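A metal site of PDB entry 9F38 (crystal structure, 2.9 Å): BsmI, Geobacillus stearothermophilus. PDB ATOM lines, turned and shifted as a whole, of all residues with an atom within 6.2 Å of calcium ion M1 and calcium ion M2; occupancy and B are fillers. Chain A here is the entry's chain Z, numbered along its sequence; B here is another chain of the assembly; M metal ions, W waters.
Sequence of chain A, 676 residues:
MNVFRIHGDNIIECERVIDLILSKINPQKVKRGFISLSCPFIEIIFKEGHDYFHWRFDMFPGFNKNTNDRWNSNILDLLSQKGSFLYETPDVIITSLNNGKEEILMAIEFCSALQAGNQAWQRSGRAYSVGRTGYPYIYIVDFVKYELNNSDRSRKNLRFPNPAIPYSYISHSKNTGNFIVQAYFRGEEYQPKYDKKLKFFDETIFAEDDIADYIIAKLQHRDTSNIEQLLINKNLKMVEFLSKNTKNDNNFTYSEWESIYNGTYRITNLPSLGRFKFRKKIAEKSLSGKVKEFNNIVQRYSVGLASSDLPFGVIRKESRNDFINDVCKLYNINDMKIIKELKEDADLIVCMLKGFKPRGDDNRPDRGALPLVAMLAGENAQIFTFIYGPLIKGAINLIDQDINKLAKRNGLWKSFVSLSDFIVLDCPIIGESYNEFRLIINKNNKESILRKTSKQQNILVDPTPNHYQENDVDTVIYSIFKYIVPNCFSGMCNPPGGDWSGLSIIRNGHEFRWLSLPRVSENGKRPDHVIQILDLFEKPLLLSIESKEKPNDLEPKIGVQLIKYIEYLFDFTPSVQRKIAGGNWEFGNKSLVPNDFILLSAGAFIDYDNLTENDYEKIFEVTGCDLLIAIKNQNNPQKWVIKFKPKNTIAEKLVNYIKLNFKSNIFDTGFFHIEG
NH2 of Arg 16 lies within salt-bridge range of OD2 of Asp 499, 3.2 Å away. The guanidinium group of Arg 123 lies within salt-bridge range of OP2 of DA 7 of chain B, 2.9 Å away. OP2 of DC 6 of chain B lies within salt-bridge range of the guanidinium group of Arg 126, 2.7 Å away. The guanidinium group (NH2) of Arg 123 is in salt-bridge range of OP2 of DC 6 of chain B, 3.3 Å away. OP2 of DG 5 of chain B lies within salt-bridge range of the guanidinium group (NH2) of Arg 126 (3.2 Å). The side-chain carboxylate (OE1) of Glu 109 is in salt-bridge range of the guanidinium group (NH1) of Arg 126. NH2 of Arg 123 sits close to OE2 of Glu 109, at 3.6 Å. The side-chain sulfur (SG) of Cys 111 lies close to the guanidinium group (NH2) of Arg 123 (3.7 Å).
Calcium ion M2 is bound by OD2 of Asp 9 (2.1 Å), OD1 of Asp 91 (2.2 Å), OP1 of DC 6 of chain B (2.8 Å) and O3' of DG 5 of chain B (2.8 Å). Calcium ion M2 has four donor atoms within binding distance. Slightly farther from calcium ion M2 lies water W1 (2.9 Å).
Arg 123 touches calcium ion M1. Asp 499 touches calcium ion M1 (OD1 to CA, 3.3 Å). Of the 18 residues printed, 6 come within 4 Å of calcium ion M1. Along chain A the residues within 4 Å of calcium ion M1 span positions 91 to 499. The nearest printed residue that does not touch calcium ion M1 is Cys 111 (4.3 Å).
Calcium ion M1 is bound by the backbone carbonyl oxygen of Phe 110 (2.1 Å), the side-chain carboxylate of Asp 91 (2.2 Å), OP1 of DC 6 of chain B (2.7 Å) and the side-chain carboxylate of Glu 109 (2.7 Å). Calcium ion M1 has four donor atoms within binding distance. Slightly farther from calcium ion M1 lies OD1 of Asp 91 (3.1 Å).
Water W1 bridges the side-chain carboxylate (OD1) of Asp 9 (2.6 Å) and the backbone carbonyl oxygen (O) of Thr 89 (3.3 Å).
Of the 18 residues printed, 4 come within 4 Å of calcium ion M2. The nearest printed residue that does not touch calcium ion M2 is Gly 497 (4.04 Å).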
ATOM      1  N   ASP A   9      24.235  14.580  14.946  1.00  0.00           N
ATOM      2  CA  ASP A   9      24.944  14.700  16.233  1.00  0.00           C
ATOM      3  C   ASP A   9      23.928  14.675  17.381  1.00  0.00           C
ATOM      4  O   ASP A   9      24.183  14.058  18.409  1.00  0.00           O
ATOM      5  CB  ASP A   9      25.708  16.036  16.316  1.00  0.00           C
ATOM      6  CG  ASP A   9      26.808  16.229  15.314  1.00  0.00           C
ATOM      7  OD1 ASP A   9      27.597  15.298  15.106  1.00  0.00           O
ATOM      8  OD2 ASP A   9      26.891  17.341  14.748  1.00  0.00           O
ATOM      9  N   GLU A  13      20.181  18.816  14.997  1.00  0.00           N
ATOM     10  CA  GLU A  13      20.815  18.680  13.689  1.00  0.00           C
ATOM     11  C   GLU A  13      19.905  17.900  12.741  1.00  0.00           C
ATOM     12  O   GLU A  13      19.761  18.276  11.590  1.00  0.00           O
ATOM     13  CB  GLU A  13      22.186  17.987  13.791  1.00  0.00           C
ATOM     14  CG  GLU A  13      23.074  18.471  14.939  1.00  0.00           C
ATOM     15  CD  GLU A  13      23.787  19.793  14.765  1.00  0.00           C
ATOM     16  OE1 GLU A  13      24.193  20.119  13.621  1.00  0.00           O
ATOM     17  OE2 GLU A  13      23.977  20.506  15.782  1.00  0.00           O
ATOM     18  N   ARG A  16      16.974  20.020  11.527  1.00  0.00           N
ATOM     19  CA  ARG A  16      17.335  21.050  10.561  1.00  0.00           C
ATOM     20  C   ARG A  16      17.190  20.555   9.125  1.00  0.00           C
ATOM     21  O   ARG A  16      16.757  21.307   8.256  1.00  0.00           O
ATOM     22  CB  ARG A  16      18.728  21.625  10.852  1.00  0.00           C
ATOM     23  CG  ARG A  16      18.738  22.489  12.101  1.00  0.00           C
ATOM     24  CD  ARG A  16      19.669  23.680  11.970  1.00  0.00           C
ATOM     25  NE  ARG A  16      21.071  23.331  12.198  1.00  0.00           N
ATOM     26  CZ  ARG A  16      21.759  23.660  13.289  1.00  0.00           C
ATOM     27  NH1 ARG A  16      21.186  24.363  14.264  1.00  0.00           N
ATOM     28  NH2 ARG A  16      23.021  23.287  13.420  1.00  0.00           N
ATOM     29  N   THR A  89      33.662  14.051  11.626  1.00  0.00           N
ATOM     30  CA  THR A  89      32.260  13.725  11.588  1.00  0.00           C
ATOM     31  C   THR A  89      31.375  14.854  11.110  1.00  0.00           C
ATOM     32  O   THR A  89      31.354  15.933  11.719  1.00  0.00           O
ATOM     33  CB  THR A  89      31.855  13.241  12.975  1.00  0.00           C
ATOM     34  OG1 THR A  89      32.654  12.108  13.314  1.00  0.00           O
ATOM     35  CG2 THR A  89      30.412  12.871  13.057  1.00  0.00           C
ATOM     36  N   PRO A  90      30.599  14.640  10.017  1.00  0.00           N
ATOM     37  CA  PRO A  90      29.665  15.684   9.572  1.00  0.00           C
ATOM     38  C   PRO A  90      28.487  15.827  10.540  1.00  0.00           C
ATOM     39  O   PRO A  90      28.287  14.966  11.396  1.00  0.00           O
ATOM     40  CB  PRO A  90      29.209  15.186   8.213  1.00  0.00           C
ATOM     41  CG  PRO A  90      29.273  13.712   8.337  1.00  0.00           C
ATOM     42  CD  PRO A  90      30.476  13.420   9.204  1.00  0.00           C
ATOM     43  N   ASP A  91      27.712  16.902  10.406  1.00  0.00           N
ATOM     44  CA  ASP A  91      26.580  17.126  11.307  1.00  0.00           C
ATOM     45  C   ASP A  91      25.450  16.136  11.052  1.00  0.00           C
ATOM     46  O   ASP A  91      24.850  15.642  12.011  1.00  0.00           O
ATOM     47  CB  ASP A  91      26.097  18.573  11.270  1.00  0.00           C
ATOM     48  CG  ASP A  91      27.068  19.565  11.898  1.00  0.00           C
ATOM     49  OD1 ASP A  91      27.989  19.129  12.630  1.00  0.00           O
ATOM     50  OD2 ASP A  91      26.913  20.776  11.658  1.00  0.00           O
ATOM     51  N   GLU A 109      26.979  19.509   6.713  1.00  0.00           N
ATOM     52  CA  GLU A 109      27.607  20.180   7.837  1.00  0.00           C
ATOM     53  C   GLU A 109      27.040  21.587   7.928  1.00  0.00           C
ATOM     54  O   GLU A 109      26.968  22.291   6.927  1.00  0.00           O
ATOM     55  CB  GLU A 109      29.125  20.219   7.648  1.00  0.00           C
ATOM     56  CG  GLU A 109      29.856  20.996   8.715  1.00  0.00           C
ATOM     57  CD  GLU A 109      30.016  20.272  10.034  1.00  0.00           C
ATOM     58  OE1 GLU A 109      29.990  19.017  10.031  1.00  0.00           O
ATOM     59  OE2 GLU A 109      30.169  20.955  11.069  1.00  0.00           O
ATOM     60  N   PHE A 110      26.598  21.990   9.116  1.00  0.00           N
ATOM     61  CA  PHE A 110      26.015  23.308   9.373  1.00  0.00           C
ATOM     62  C   PHE A 110      27.014  24.149  10.172  1.00  0.00           C
ATOM     63  O   PHE A 110      27.413  23.722  11.251  1.00  0.00           O
ATOM     64  CB  PHE A 110      24.737  23.155  10.219  1.00  0.00           C
ATOM     65  CG  PHE A 110      23.708  22.174   9.705  1.00  0.00           C
ATOM     66  CD1 PHE A 110      23.160  22.321   8.452  1.00  0.00           C
ATOM     67  CD2 PHE A 110      23.277  21.124  10.492  1.00  0.00           C
ATOM     68  CE1 PHE A 110      22.189  21.446   8.000  1.00  0.00           C
ATOM     69  CE2 PHE A 110      22.293  20.259  10.034  1.00  0.00           C
ATOM     70  CZ  PHE A 110      21.760  20.429   8.807  1.00  0.00           C
ATOM     71  N   CYS A 111      27.402  25.329   9.667  1.00  0.00           N
ATOM     72  CA  CYS A 111      28.360  26.165  10.394  1.00  0.00           C
ATOM     73  C   CYS A 111      27.914  27.608  10.547  1.00  0.00           C
ATOM     74  O   CYS A 111      27.933  28.375   9.601  1.00  0.00           O
ATOM     75  CB  CYS A 111      29.751  26.086   9.769  1.00  0.00           C
ATOM     76  SG  CYS A 111      31.087  26.682  10.850  1.00  0.00           S
ATOM     77  N   SER A 112      27.573  27.971  11.774  1.00  0.00           N
ATOM     78  CA  SER A 112      27.205  29.346  12.106  1.00  0.00           C
ATOM     79  C   SER A 112      28.418  30.181  12.481  1.00  0.00           C
ATOM     80  O   SER A 112      28.425  31.397  12.251  1.00  0.00           O
ATOM     81  CB  SER A 112      26.196  29.352  13.244  1.00  0.00           C
ATOM     82  OG  SER A 112      24.923  29.604  12.668  1.00  0.00           O
ATOM     83  N   ARG A 123      37.005  22.772   9.676  1.00  0.00           N
ATOM     84  CA  ARG A 123      36.271  21.581   9.284  1.00  0.00           C
ATOM     85  C   ARG A 123      36.427  21.251   7.793  1.00  0.00           C
ATOM     86  O   ARG A 123      35.513  20.722   7.173  1.00  0.00           O
ATOM     87  CB  ARG A 123      34.795  21.611   9.712  1.00  0.00           C
ATOM     88  CG  ARG A 123      34.116  22.960   9.720  1.00  0.00           C
ATOM     89  CD  ARG A 123      32.942  22.885  10.712  1.00  0.00           C
ATOM     90  NE  ARG A 123      33.290  23.825  11.733  1.00  0.00           N
ATOM     91  CZ  ARG A 123      32.607  24.251  12.778  1.00  0.00           C
ATOM     92  NH1 ARG A 123      33.123  25.172  13.584  1.00  0.00           N
ATOM     93  NH2 ARG A 123      31.403  23.758  13.046  1.00  0.00           N
ATOM     94  N   ARG A 126      36.634  17.104   7.077  1.00  0.00           N
ATOM     95  CA  ARG A 126      35.454  16.311   6.723  1.00  0.00           C
ATOM     96  C   ARG A 126      35.099  16.502   5.281  1.00  0.00           C
ATOM     97  O   ARG A 126      34.766  15.527   4.631  1.00  0.00           O
ATOM     98  CB  ARG A 126      34.256  16.527   7.660  1.00  0.00           C
ATOM     99  CG  ARG A 126      33.954  17.960   8.008  1.00  0.00           C
ATOM    100  CD  ARG A 126      33.099  18.039   9.253  1.00  0.00           C
ATOM    101  NE  ARG A 126      33.904  17.767  10.433  1.00  0.00           N
ATOM    102  CZ  ARG A 126      33.881  18.489  11.558  1.00  0.00           C
ATOM    103  NH1 ARG A 126      33.017  19.485  11.687  1.00  0.00           N
ATOM    104  NH2 ARG A 126      34.687  18.190  12.567  1.00  0.00           N
ATOM    105  N   GLY A 497      27.336  18.134  21.834  1.00  0.00           N
ATOM    106  CA  GLY A 497      27.944  18.218  20.515  1.00  0.00           C
ATOM    107  C   GLY A 497      27.184  19.108  19.558  1.00  0.00           C
ATOM    108  O   GLY A 497      27.176  18.865  18.353  1.00  0.00           O
ATOM    109  N   GLY A 498      26.558  20.146  20.083  1.00  0.00           N
ATOM    110  CA  GLY A 498      25.752  21.055  19.296  1.00  0.00           C
ATOM    111  C   GLY A 498      26.383  22.396  18.980  1.00  0.00           C
ATOM    112  O   GLY A 498      27.313  22.831  19.652  1.00  0.00           O
ATOM    113  N   ASP A 499      25.828  23.064  17.955  1.00  0.00           N
ATOM    114  CA  ASP A 499      26.256  24.376  17.465  1.00  0.00           C
ATOM    115  C   ASP A 499      25.942  25.508  18.457  1.00  0.00           C
ATOM    116  O   ASP A 499      25.199  25.320  19.408  1.00  0.00           O
ATOM    117  CB  ASP A 499      25.552  24.674  16.116  1.00  0.00           C
ATOM    118  CG  ASP A 499      26.031  23.860  14.934  1.00  0.00           C
ATOM    119  OD1 ASP A 499      26.374  22.678  15.127  1.00  0.00           O
ATOM    120  OD2 ASP A 499      26.033  24.408  13.803  1.00  0.00           O
ATOM    121  P    DG B   5      35.770  16.015  14.562  1.00  0.00           P
ATOM    122  OP1  DG B   5      35.286  15.085  13.521  1.00  0.00           O
ATOM    123  OP2  DG B   5      37.006  16.805  14.345  1.00  0.00           O
ATOM    124  O5'  DG B   5      34.594  17.035  14.938  1.00  0.00           O
ATOM    125  C5'  DG B   5      33.242  16.590  15.035  1.00  0.00           C
ATOM    126  C4'  DG B   5      32.524  17.236  16.211  1.00  0.00           C
ATOM    127  O4'  DG B   5      33.262  16.979  17.435  1.00  0.00           O
ATOM    128  C3'  DG B   5      32.408  18.749  16.173  1.00  0.00           C
ATOM    129  O3'  DG B   5      31.318  19.168  15.344  1.00  0.00           O
ATOM    130  C2'  DG B   5      32.116  19.034  17.634  1.00  0.00           C
ATOM    131  C1'  DG B   5      33.047  18.056  18.333  1.00  0.00           C
ATOM    132  N9   DG B   5      34.325  18.650  18.707  1.00  0.00           N
ATOM    133  C8   DG B   5      35.517  18.573  18.026  1.00  0.00           C
ATOM    134  N7   DG B   5      36.479  19.244  18.600  1.00  0.00           N
ATOM    135  C5   DG B   5      35.856  19.876  19.665  1.00  0.00           C
ATOM    136  C6   DG B   5      36.373  20.778  20.626  1.00  0.00           C
ATOM    137  O6   DG B   5      37.532  21.202  20.727  1.00  0.00           O
ATOM    138  N1   DG B   5      35.395  21.181  21.526  1.00  0.00           N
ATOM    139  C2   DG B   5      34.079  20.791  21.485  1.00  0.00           C
ATOM    140  N2   DG B   5      33.282  21.270  22.443  1.00  0.00           N
ATOM    141  N3   DG B   5      33.592  19.938  20.608  1.00  0.00           N
ATOM    142  C4   DG B   5      34.526  19.530  19.723  1.00  0.00           C
ATOM    143  P    DC B   6      31.329  20.624  14.667  1.00  0.00           P
ATOM    144  OP1  DC B   6      30.118  20.731  13.826  1.00  0.00           O
ATOM    145  OP2  DC B   6      32.669  20.836  14.054  1.00  0.00           O
ATOM    146  O5'  DC B   6      31.199  21.630  15.902  1.00  0.00           O
ATOM    147  C5'  DC B   6      30.049  21.584  16.754  1.00  0.00           C
ATOM    148  C4'  DC B   6      30.188  22.538  17.934  1.00  0.00           C
ATOM    149  O4'  DC B   6      31.270  22.113  18.799  1.00  0.00           O
ATOM    150  C3'  DC B   6      30.552  23.957  17.569  1.00  0.00           C
ATOM    151  O3'  DC B   6      29.432  24.687  17.139  1.00  0.00           O
ATOM    152  C2'  DC B   6      31.094  24.483  18.889  1.00  0.00           C
ATOM    153  C1'  DC B   6      31.849  23.261  19.418  1.00  0.00           C
ATOM    154  N1   DC B   6      33.322  23.313  19.132  1.00  0.00           N
ATOM    155  C2   DC B   6      34.178  24.040  19.957  1.00  0.00           C
ATOM    156  O2   DC B   6      33.706  24.591  20.957  1.00  0.00           O
ATOM    157  N3   DC B   6      35.497  24.089  19.664  1.00  0.00           N
ATOM    158  C4   DC B   6      35.956  23.473  18.580  1.00  0.00           C
ATOM    159  N4   DC B   6      37.262  23.551  18.314  1.00  0.00           N
ATOM    160  C5   DC B   6      35.115  22.752  17.707  1.00  0.00           C
ATOM    161  C6   DC B   6      33.815  22.688  18.017  1.00  0.00           C
ATOM    162  P    DA B   7      29.655  25.953  16.197  1.00  0.00           P
ATOM    163  OP1  DA B   7      28.396  26.206  15.451  1.00  0.00           O
ATOM    164  OP2  DA B   7      30.919  25.735  15.460  1.00  0.00           O
ATOM    165  O5'  DA B   7      29.874  27.134  17.265  1.00  0.00           O
ATOM    166  C5'  DA B   7      30.860  28.123  17.040  1.00  0.00           C
ATOM    167  C4'  DA B   7      31.506  28.544  18.331  1.00  0.00           C
ATOM    168  O4'  DA B   7      32.498  27.570  18.716  1.00  0.00           O
ATOM    169  C3'  DA B   7      32.242  29.858  18.227  1.00  0.00           C
ATOM    170  O3'  DA B   7      31.358  30.878  18.622  1.00  0.00           O
ATOM    171  C2'  DA B   7      33.396  29.706  19.213  1.00  0.00           C
ATOM    172  C1'  DA B   7      33.618  28.200  19.295  1.00  0.00           C
ATOM    173  N9   DA B   7      34.806  27.726  18.599  1.00  0.00           N
ATOM    174  C8   DA B   7      34.841  26.930  17.500  1.00  0.00           C
ATOM    175  N7   DA B   7      36.049  26.601  17.116  1.00  0.00           N
ATOM    176  C5   DA B   7      36.866  27.211  18.059  1.00  0.00           C
ATOM    177  C6   DA B   7      38.260  27.223  18.222  1.00  0.00           C
ATOM    178  N6   DA B   7      39.101  26.602  17.402  1.00  0.00           N
ATOM    179  N1   DA B   7      38.758  27.913  19.265  1.00  0.00           N
ATOM    180  C2   DA B   7      37.905  28.545  20.079  1.00  0.00           C
ATOM    181  N3   DA B   7      36.575  28.595  20.037  1.00  0.00           N
ATOM    182  C4   DA B   7      36.112  27.899  18.980  1.00  0.00           C
HETATM  183 CA    CA M   1      28.314  22.258  12.533  1.00  0.00          CA
HETATM  184 CA    CA M   2      28.674  18.439  14.630  1.00  0.00          CA
HETATM  185  O   HOH W   1      30.060  15.880  14.791  1.00  0.00           O
